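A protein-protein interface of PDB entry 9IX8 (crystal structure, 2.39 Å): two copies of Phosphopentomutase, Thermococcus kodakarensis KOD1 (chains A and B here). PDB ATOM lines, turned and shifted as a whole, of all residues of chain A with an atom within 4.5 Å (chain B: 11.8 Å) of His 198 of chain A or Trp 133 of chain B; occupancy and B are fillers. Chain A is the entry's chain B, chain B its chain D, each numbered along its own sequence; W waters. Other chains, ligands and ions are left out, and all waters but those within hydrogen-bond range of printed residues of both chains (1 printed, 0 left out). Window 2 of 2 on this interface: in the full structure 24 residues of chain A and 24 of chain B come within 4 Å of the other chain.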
ATOM      1  N   LEU A  12      15.641  23.018 -27.416  1.00  0.00           N
ATOM      2  CA  LEU A  12      14.412  22.205 -27.250  1.00  0.00           C
ATOM      3  C   LEU A  12      14.413  21.081 -28.276  1.00  0.00           C
ATOM      4  O   LEU A  12      14.708  21.375 -29.426  1.00  0.00           O
ATOM      5  CB  LEU A  12      13.169  23.090 -27.431  1.00  0.00           C
ATOM      6  CG  LEU A  12      11.954  22.689 -26.591  1.00  0.00           C
ATOM      7  CD1 LEU A  12      12.243  22.879 -25.117  1.00  0.00           C
ATOM      8  CD2 LEU A  12      10.724  23.483 -26.983  1.00  0.00           C
ATOM      9  N   THR A  44       8.970  29.959 -23.361  1.00  0.00           N
ATOM     10  CA  THR A  44       7.673  29.339 -23.677  1.00  0.00           C
ATOM     11  C   THR A  44       7.650  27.889 -23.242  1.00  0.00           C
ATOM     12  O   THR A  44       6.570  27.343 -23.209  1.00  0.00           O
ATOM     13  CB  THR A  44       7.419  29.406 -25.165  1.00  0.00           C
ATOM     14  OG1 THR A  44       8.483  28.621 -25.715  1.00  0.00           O
ATOM     15  CG2 THR A  44       7.389  30.836 -25.673  1.00  0.00           C
ATOM     16  N   PRO A  96      14.994  32.150 -27.747  1.00  0.00           N
ATOM     17  CA  PRO A  96      13.746  31.526 -27.332  1.00  0.00           C
ATOM     18  C   PRO A  96      13.645  30.018 -27.607  1.00  0.00           C
ATOM     19  O   PRO A  96      12.826  29.396 -26.990  1.00  0.00           O
ATOM     20  CB  PRO A  96      12.678  32.303 -28.135  1.00  0.00           C
ATOM     21  CG  PRO A  96      13.439  33.107 -29.173  1.00  0.00           C
ATOM     22  CD  PRO A  96      14.762  33.396 -28.502  1.00  0.00           C
ATOM     23  N   THR A  97      14.442  29.481 -28.535  1.00  0.00           N
ATOM     24  CA  THR A  97      14.442  28.049 -28.962  1.00  0.00           C
ATOM     25  C   THR A  97      15.045  27.144 -27.877  1.00  0.00           C
ATOM     26  O   THR A  97      14.974  25.937 -28.029  1.00  0.00           O
ATOM     27  CB  THR A  97      15.294  27.885 -30.231  1.00  0.00           C
ATOM     28  OG1 THR A  97      16.517  28.558 -29.936  1.00  0.00           O
ATOM     29  CG2 THR A  97      14.665  28.489 -31.466  1.00  0.00           C
ATOM     30  N   ASP A 196       7.840  37.911 -21.439  1.00  0.00           N
ATOM     31  CA  ASP A 196       7.472  37.303 -22.738  1.00  0.00           C
ATOM     32  C   ASP A 196       8.629  36.432 -23.231  1.00  0.00           C
ATOM     33  O   ASP A 196       9.718  36.987 -23.524  1.00  0.00           O
ATOM     34  CB  ASP A 196       7.135  38.400 -23.756  1.00  0.00           C
ATOM     35  CG  ASP A 196       6.444  37.891 -25.004  1.00  0.00           C
ATOM     36  OD1 ASP A 196       6.696  36.726 -25.374  1.00  0.00           O
ATOM     37  OD2 ASP A 196       5.621  38.643 -25.556  1.00  0.00           O
ATOM     38  N   GLY A 197       8.363  35.135 -23.397  1.00  0.00           N
ATOM     39  CA  GLY A 197       9.332  34.113 -23.835  1.00  0.00           C
ATOM     40  C   GLY A 197       9.578  34.085 -25.333  1.00  0.00           C
ATOM     41  O   GLY A 197      10.296  33.193 -25.760  1.00  0.00           O
ATOM     42  N   HIS A 198       9.043  35.030 -26.106  1.00  0.00           N
ATOM     43  CA  HIS A 198       9.437  35.259 -27.525  1.00  0.00           C
ATOM     44  C   HIS A 198      10.547  36.325 -27.540  1.00  0.00           C
ATOM     45  O   HIS A 198      11.117  36.574 -28.590  1.00  0.00           O
ATOM     46  CB  HIS A 198       8.231  35.624 -28.405  1.00  0.00           C
ATOM     47  CG  HIS A 198       7.119  34.625 -28.470  1.00  0.00           C
ATOM     48  ND1 HIS A 198       6.500  34.302 -29.654  1.00  0.00           N
ATOM     49  CD2 HIS A 198       6.442  33.941 -27.513  1.00  0.00           C
ATOM     50  CE1 HIS A 198       5.517  33.432 -29.437  1.00  0.00           C
ATOM     51  NE2 HIS A 198       5.452  33.189 -28.129  1.00  0.00           N
ATOM     52  N   PHE A 199      10.901  36.877 -26.387  1.00  0.00           N
ATOM     53  CA  PHE A 199      11.941  37.934 -26.246  1.00  0.00           C
ATOM     54  C   PHE A 199      11.767  38.968 -27.362  1.00  0.00           C
ATOM     55  O   PHE A 199      12.708  39.298 -28.082  1.00  0.00           O
ATOM     56  CB  PHE A 199      13.341  37.306 -26.221  1.00  0.00           C
ATOM     57  CG  PHE A 199      13.633  36.498 -24.984  1.00  0.00           C
ATOM     58  CD1 PHE A 199      13.727  37.104 -23.746  1.00  0.00           C
ATOM     59  CD2 PHE A 199      13.779  35.124 -25.046  1.00  0.00           C
ATOM     60  CE1 PHE A 199      13.955  36.359 -22.600  1.00  0.00           C
ATOM     61  CE2 PHE A 199      14.036  34.386 -23.903  1.00  0.00           C
ATOM     62  CZ  PHE A 199      14.121  35.005 -22.683  1.00  0.00           C
ATOM     63  N   PRO A 200      10.558  39.549 -27.526  1.00  0.00           N
ATOM     64  CA  PRO A 200      10.271  40.392 -28.688  1.00  0.00           C
ATOM     65  C   PRO A 200      11.165  41.639 -28.719  1.00  0.00           C
ATOM     66  O   PRO A 200      11.548  42.060 -29.770  1.00  0.00           O
ATOM     67  CB  PRO A 200       8.799  40.763 -28.474  1.00  0.00           C
ATOM     68  CG  PRO A 200       8.640  40.726 -26.969  1.00  0.00           C
ATOM     69  CD  PRO A 200       9.439  39.506 -26.566  1.00  0.00           C
ATOM     70  N   SER B  55       3.157  17.915 -18.606  1.00  0.00           N
ATOM     71  CA  SER B  55       4.441  18.091 -19.316  1.00  0.00           C
ATOM     72  C   SER B  55       4.328  17.480 -20.725  1.00  0.00           C
ATOM     73  O   SER B  55       4.644  18.170 -21.694  1.00  0.00           O
ATOM     74  CB  SER B  55       5.525  17.509 -18.563  1.00  0.00           C
ATOM     75  OG  SER B  55       6.749  17.966 -19.081  1.00  0.00           O
ATOM     76  N   LEU B  57       1.353  16.614 -22.438  1.00  0.00           N
ATOM     77  CA  LEU B  57       0.294  17.301 -23.208  1.00  0.00           C
ATOM     78  C   LEU B  57       0.877  18.629 -23.739  1.00  0.00           C
ATOM     79  O   LEU B  57       0.918  18.842 -24.956  1.00  0.00           O
ATOM     80  CB  LEU B  57      -0.911  17.445 -22.275  1.00  0.00           C
ATOM     81  CG  LEU B  57      -1.763  16.191 -22.049  1.00  0.00           C
ATOM     82  CD1 LEU B  57      -2.804  16.415 -20.948  1.00  0.00           C
ATOM     83  CD2 LEU B  57      -2.480  15.751 -23.302  1.00  0.00           C
ATOM     84  N   LEU B  58       1.405  19.481 -22.875  1.00  0.00           N
ATOM     85  CA  LEU B  58       2.099  20.732 -23.296  1.00  0.00           C
ATOM     86  C   LEU B  58       3.095  20.477 -24.445  1.00  0.00           C
ATOM     87  O   LEU B  58       3.190  21.310 -25.329  1.00  0.00           O
ATOM     88  CB  LEU B  58       2.812  21.346 -22.090  1.00  0.00           C
ATOM     89  CG  LEU B  58       1.878  21.983 -21.058  1.00  0.00           C
ATOM     90  CD1 LEU B  58       2.674  22.642 -19.924  1.00  0.00           C
ATOM     91  CD2 LEU B  58       0.959  22.988 -21.730  1.00  0.00           C
ATOM     92  N   SER B  59       3.832  19.373 -24.431  1.00  0.00           N
ATOM     93  CA  SER B  59       4.944  19.157 -25.397  1.00  0.00           C
ATOM     94  C   SER B  59       4.382  19.010 -26.822  1.00  0.00           C
ATOM     95  O   SER B  59       5.127  19.321 -27.760  1.00  0.00           O
ATOM     96  CB  SER B  59       5.736  17.977 -25.048  1.00  0.00           C
ATOM     97  OG  SER B  59       5.185  16.844 -25.695  1.00  0.00           O
ATOM     98  N   THR B  60       3.125  18.578 -26.957  1.00  0.00           N
ATOM     99  CA  THR B  60       2.440  18.359 -28.260  1.00  0.00           C
ATOM    100  C   THR B  60       1.729  19.619 -28.802  1.00  0.00           C
ATOM    101  O   THR B  60       1.166  19.536 -29.941  1.00  0.00           O
ATOM    102  CB  THR B  60       1.378  17.260 -28.133  1.00  0.00           C
ATOM    103  OG1 THR B  60       0.289  17.857 -27.435  1.00  0.00           O
ATOM    104  CG2 THR B  60       1.859  16.036 -27.398  1.00  0.00           C
ATOM    105  N   GLY B  61       1.700  20.743 -28.069  1.00  0.00           N
ATOM    106  CA  GLY B  61       0.996  21.965 -28.519  1.00  0.00           C
ATOM    107  C   GLY B  61      -0.462  22.069 -28.066  1.00  0.00           C
ATOM    108  O   GLY B  61      -1.094  23.101 -28.358  1.00  0.00           O
ATOM    109  N   MET B  62      -1.019  21.051 -27.420  1.00  0.00           N
ATOM    110  CA  MET B  62      -2.363  21.132 -26.796  1.00  0.00           C
ATOM    111  C   MET B  62      -2.373  22.222 -25.714  1.00  0.00           C
ATOM    112  O   MET B  62      -1.355  22.450 -25.044  1.00  0.00           O
ATOM    113  CB  MET B  62      -2.775  19.800 -26.165  1.00  0.00           C
ATOM    114  CG  MET B  62      -3.183  18.749 -27.160  1.00  0.00           C
ATOM    115  SD  MET B  62      -4.213  17.461 -26.377  1.00  0.00           S
ATOM    116  CE  MET B  62      -5.839  18.175 -26.566  1.00  0.00           C
ATOM    117  N   ARG B 129       3.860  13.921 -31.689  1.00  0.00           N
ATOM    118  CA  ARG B 129       3.780  15.303 -32.183  1.00  0.00           C
ATOM    119  C   ARG B 129       4.525  16.191 -31.187  1.00  0.00           C
ATOM    120  O   ARG B 129       4.282  16.065 -29.993  1.00  0.00           O
ATOM    121  CB  ARG B 129       2.321  15.667 -32.359  1.00  0.00           C
ATOM    122  CG  ARG B 129       2.088  17.016 -32.999  1.00  0.00           C
ATOM    123  CD  ARG B 129       0.729  17.414 -32.512  1.00  0.00           C
ATOM    124  NE  ARG B 129      -0.143  17.700 -33.605  1.00  0.00           N
ATOM    125  CZ  ARG B 129      -1.438  17.422 -33.645  1.00  0.00           C
ATOM    126  NH1 ARG B 129      -2.032  16.814 -32.623  1.00  0.00           N
ATOM    127  NH2 ARG B 129      -2.109  17.734 -34.754  1.00  0.00           N
ATOM    128  N   LYS B 130       5.504  16.933 -31.692  1.00  0.00           N
ATOM    129  CA  LYS B 130       6.295  17.935 -30.969  1.00  0.00           C
ATOM    130  C   LYS B 130       5.879  19.312 -31.491  1.00  0.00           C
ATOM    131  O   LYS B 130       5.867  19.525 -32.733  1.00  0.00           O
ATOM    132  CB  LYS B 130       7.781  17.658 -31.172  1.00  0.00           C
ATOM    133  CG  LYS B 130       8.284  16.344 -30.567  1.00  0.00           C
ATOM    134  CD  LYS B 130       8.336  16.307 -29.037  1.00  0.00           C
ATOM    135  CE  LYS B 130       8.672  14.959 -28.417  1.00  0.00           C
ATOM    136  NZ  LYS B 130      10.046  14.508 -28.761  1.00  0.00           N
ATOM    137  N   ALA B 131       5.544  20.221 -30.580  1.00  0.00           N
ATOM    138  CA  ALA B 131       5.227  21.637 -30.877  1.00  0.00           C
ATOM    139  C   ALA B 131       6.532  22.362 -31.206  1.00  0.00           C
ATOM    140  O   ALA B 131       7.536  21.962 -30.680  1.00  0.00           O
ATOM    141  CB  ALA B 131       4.530  22.267 -29.702  1.00  0.00           C
ATOM    142  N   ARG B 132       6.528  23.396 -32.040  1.00  0.00           N
ATOM    143  CA  ARG B 132       7.656  24.372 -32.012  1.00  0.00           C
ATOM    144  C   ARG B 132       7.600  25.134 -30.681  1.00  0.00           C
ATOM    145  O   ARG B 132       6.495  25.331 -30.119  1.00  0.00           O
ATOM    146  CB  ARG B 132       7.613  25.378 -33.163  1.00  0.00           C
ATOM    147  CG  ARG B 132       7.511  24.785 -34.566  1.00  0.00           C
ATOM    148  CD  ARG B 132       6.839  25.800 -35.482  1.00  0.00           C
ATOM    149  NE  ARG B 132       7.500  27.088 -35.294  1.00  0.00           N
ATOM    150  CZ  ARG B 132       8.647  27.442 -35.871  1.00  0.00           C
ATOM    151  NH1 ARG B 132       9.261  26.636 -36.726  1.00  0.00           N
ATOM    152  NH2 ARG B 132       9.167  28.625 -35.607  1.00  0.00           N
ATOM    153  N   TRP B 133       8.758  25.586 -30.213  1.00  0.00           N
ATOM    154  CA  TRP B 133       8.884  26.416 -28.989  1.00  0.00           C
ATOM    155  C   TRP B 133       7.759  27.457 -28.914  1.00  0.00           C
ATOM    156  O   TRP B 133       7.267  27.682 -27.769  1.00  0.00           O
ATOM    157  CB  TRP B 133      10.263  27.072 -28.877  1.00  0.00           C
ATOM    158  CG  TRP B 133      10.507  28.154 -29.879  1.00  0.00           C
ATOM    159  CD1 TRP B 133      11.081  28.004 -31.111  1.00  0.00           C
ATOM    160  CD2 TRP B 133      10.220  29.557 -29.737  1.00  0.00           C
ATOM    161  NE1 TRP B 133      11.163  29.212 -31.746  1.00  0.00           N
ATOM    162  CE2 TRP B 133      10.634  30.184 -30.939  1.00  0.00           C
ATOM    163  CE3 TRP B 133       9.633  30.343 -28.736  1.00  0.00           C
ATOM    164  CZ2 TRP B 133      10.466  31.554 -31.167  1.00  0.00           C
ATOM    165  CZ3 TRP B 133       9.504  31.699 -28.950  1.00  0.00           C
ATOM    166  CH2 TRP B 133       9.912  32.298 -30.148  1.00  0.00           C
ATOM    167  N   ASP B 134       7.396  28.086 -30.047  1.00  0.00           N
ATOM    168  CA  ASP B 134       6.477  29.262 -30.088  1.00  0.00           C
ATOM    169  C   ASP B 134       5.009  28.817 -30.221  1.00  0.00           C
ATOM    170  O   ASP B 134       4.144  29.710 -30.381  1.00  0.00           O
ATOM    171  CB  ASP B 134       6.879  30.272 -31.173  1.00  0.00           C
ATOM    172  CG  ASP B 134       6.815  29.816 -32.634  1.00  0.00           C
ATOM    173  OD1 ASP B 134       6.687  28.618 -32.926  1.00  0.00           O
ATOM    174  OD2 ASP B 134       6.914  30.681 -33.485  1.00  0.00           O
ATOM    175  N   GLU B 135       4.731  27.515 -30.174  1.00  0.00           N
ATOM    176  CA  GLU B 135       3.361  26.927 -30.196  1.00  0.00           C
ATOM    177  C   GLU B 135       3.008  26.337 -28.810  1.00  0.00           C
ATOM    178  O   GLU B 135       1.953  25.685 -28.686  1.00  0.00           O
ATOM    179  CB  GLU B 135       3.292  25.814 -31.247  1.00  0.00           C
ATOM    180  CG  GLU B 135       3.425  26.304 -32.691  1.00  0.00           C
ATOM    181  CD  GLU B 135       3.591  25.211 -33.755  1.00  0.00           C
ATOM    182  OE1 GLU B 135       2.956  25.325 -34.802  1.00  0.00           O
ATOM    183  OE2 GLU B 135       4.326  24.218 -33.523  1.00  0.00           O
ATOM    184  N   ILE B 136       3.889  26.451 -27.807  1.00  0.00           N
ATOM    185  CA  ILE B 136       3.635  25.815 -26.482  1.00  0.00           C
ATOM    186  C   ILE B 136       2.643  26.713 -25.738  1.00  0.00           C
ATOM    187  O   ILE B 136       2.971  27.844 -25.506  1.00  0.00           O
ATOM    188  CB  ILE B 136       4.936  25.538 -25.687  1.00  0.00           C
ATOM    189  CG1 ILE B 136       5.795  24.509 -26.432  1.00  0.00           C
ATOM    190  CG2 ILE B 136       4.600  25.075 -24.253  1.00  0.00           C
ATOM    191  CD1 ILE B 136       7.169  24.352 -25.876  1.00  0.00           C
ATOM    192  N   LYS B 137       1.448  26.234 -25.422  1.00  0.00           N
ATOM    193  CA  LYS B 137       0.384  27.110 -24.855  1.00  0.00           C
ATOM    194  C   LYS B 137       0.505  27.173 -23.328  1.00  0.00           C
ATOM    195  O   LYS B 137       0.940  26.232 -22.659  1.00  0.00           O
ATOM    196  CB  LYS B 137      -0.946  26.687 -25.484  1.00  0.00           C
ATOM    197  CG  LYS B 137      -1.049  27.146 -26.939  1.00  0.00           C
ATOM    198  CD  LYS B 137      -1.987  26.354 -27.832  1.00  0.00           C
ATOM    199  CE  LYS B 137      -1.650  26.482 -29.309  1.00  0.00           C
ATOM    200  NZ  LYS B 137      -0.694  25.447 -29.801  1.00  0.00           N
ATOM    201  N   PRO B 138       0.271  28.359 -22.728  1.00  0.00           N
ATOM    202  CA  PRO B 138       0.210  28.489 -21.275  1.00  0.00           C
ATOM    203  C   PRO B 138      -0.940  27.675 -20.669  1.00  0.00           C
ATOM    204  O   PRO B 138      -1.978  27.549 -21.295  1.00  0.00           O
ATOM    205  CB  PRO B 138      -0.066  29.992 -21.032  1.00  0.00           C
ATOM    206  CG  PRO B 138       0.317  30.693 -22.319  1.00  0.00           C
ATOM    207  CD  PRO B 138       0.120  29.660 -23.404  1.00  0.00           C
ATOM    208  N   VAL B 139      -0.700  27.089 -19.486  1.00  0.00           N
ATOM    209  CA  VAL B 139      -1.728  26.356 -18.692  1.00  0.00           C
ATOM    210  C   VAL B 139      -2.770  27.407 -18.252  1.00  0.00           C
ATOM    211  O   VAL B 139      -2.376  28.579 -18.078  1.00  0.00           O
ATOM    212  CB  VAL B 139      -1.070  25.626 -17.500  1.00  0.00           C
ATOM    213  CG1 VAL B 139      -2.070  25.062 -16.500  1.00  0.00           C
ATOM    214  CG2 VAL B 139      -0.148  24.527 -18.007  1.00  0.00           C
HETATM  215  O   HOH W   1       4.113  28.945 -23.214  1.00  0.00           O
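The side-chain hydroxyl (OG1) of Thr 44 of chain A sits at hydrogen-bond distance from the backbone carbonyl oxygen (O) of Trp 133 of chain B, at 2.6 Å.
N of Leu 12 of chain A sits at hydrogen-bond distance from O of Thr 97 of chain A, at 3.1 Å.
The backbone NH (N) of His 198 of chain A lies within hydrogen-bond range of the side-chain carboxylate (OD1) of Asp 196 of chain A (3.0 Å).
The guanidinium group of Arg 132 of chain B lies within salt-bridge range of the side-chain carboxylate of Asp 134 of chain B, 2.9 Å away.
Ile 136 of chain B touches Leu 12 of chain A.
Thr 44 of chain A touches Ile 136 of chain B (O to CG2, 3.2 Å).
CZ3 of Trp 133 of chain B touches CB of Pro 96 of chain A, 3.3 Å away.
Thr 97 of chain A touches Trp 133 of chain B (CG2 to NE1, 3.6 Å).
Gly 197 of chain A touches Trp 133 of chain B (O to CZ3, 3.6 Å).
His 198 of chain A touches Trp 133 of chain B.
CE1 of His 198 of chain A touches CB of Asp 134 of chain B, 3.9 Å away.
Printed residues of chain B within 4 Å of Leu 12 of chain A: Ile 136 (3.8 Å).
Of chain B, only Trp 133 and Ile 136 come within 4 Å of Thr 44 of chain A.
Of the printed residues of chain B, Pro 96 of chain A touches Trp 133.
Thr 97 of chain A touches just one residue of chain B: Trp 133 (3.6 Å).
No residue of chain B comes within 4 Å of Asp 196 of chain A.
Of chain B, only Trp 133 and Asp 134 come within 4 Å of His 198 of chain A.
No residue of chain B comes within 4 Å of Phe 199 of chain A.
Printed residues of chain A within 4 Å of Trp 133 of chain B: Thr 44 (2.6 Å), Pro 96 (3.3 Å), Thr 97 (3.6 Å), Gly 197 (3.6 Å) and His 198 (3.8 Å).
Printed residues of chain A within 4 Å of Asp 134 of chain B: His 198.
Printed residues of chain A within 4 Å of Ile 136 of chain B: Leu 12 (3.8 Å) and Thr 44 (3.2 Å).
The nearest residue of chain B that does not touch His 198 of chain A is Glu 135 of chain B (6.0 Å).
The nearest printed residue of chain A that does not touch Trp 133 of chain B is Leu 12 of chain A (4.002 Å).
Of the 9 printed residues of chain A, 6 touch a printed residue of chain B.
Among the printed residues, no Asp or Glu carboxylate lies within 4 Å of a Lys or Arg side-chain nitrogen of the other chain.
No position is printed for both chains.
Of the 8 pairs that touch across the chains among the printed residues, none has its exchanged pair printed and touching as well.
Water W1 bridges O of Ile 136 of chain B (2.8 Å) and O of Thr 44 of chain A (2.9 Å).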
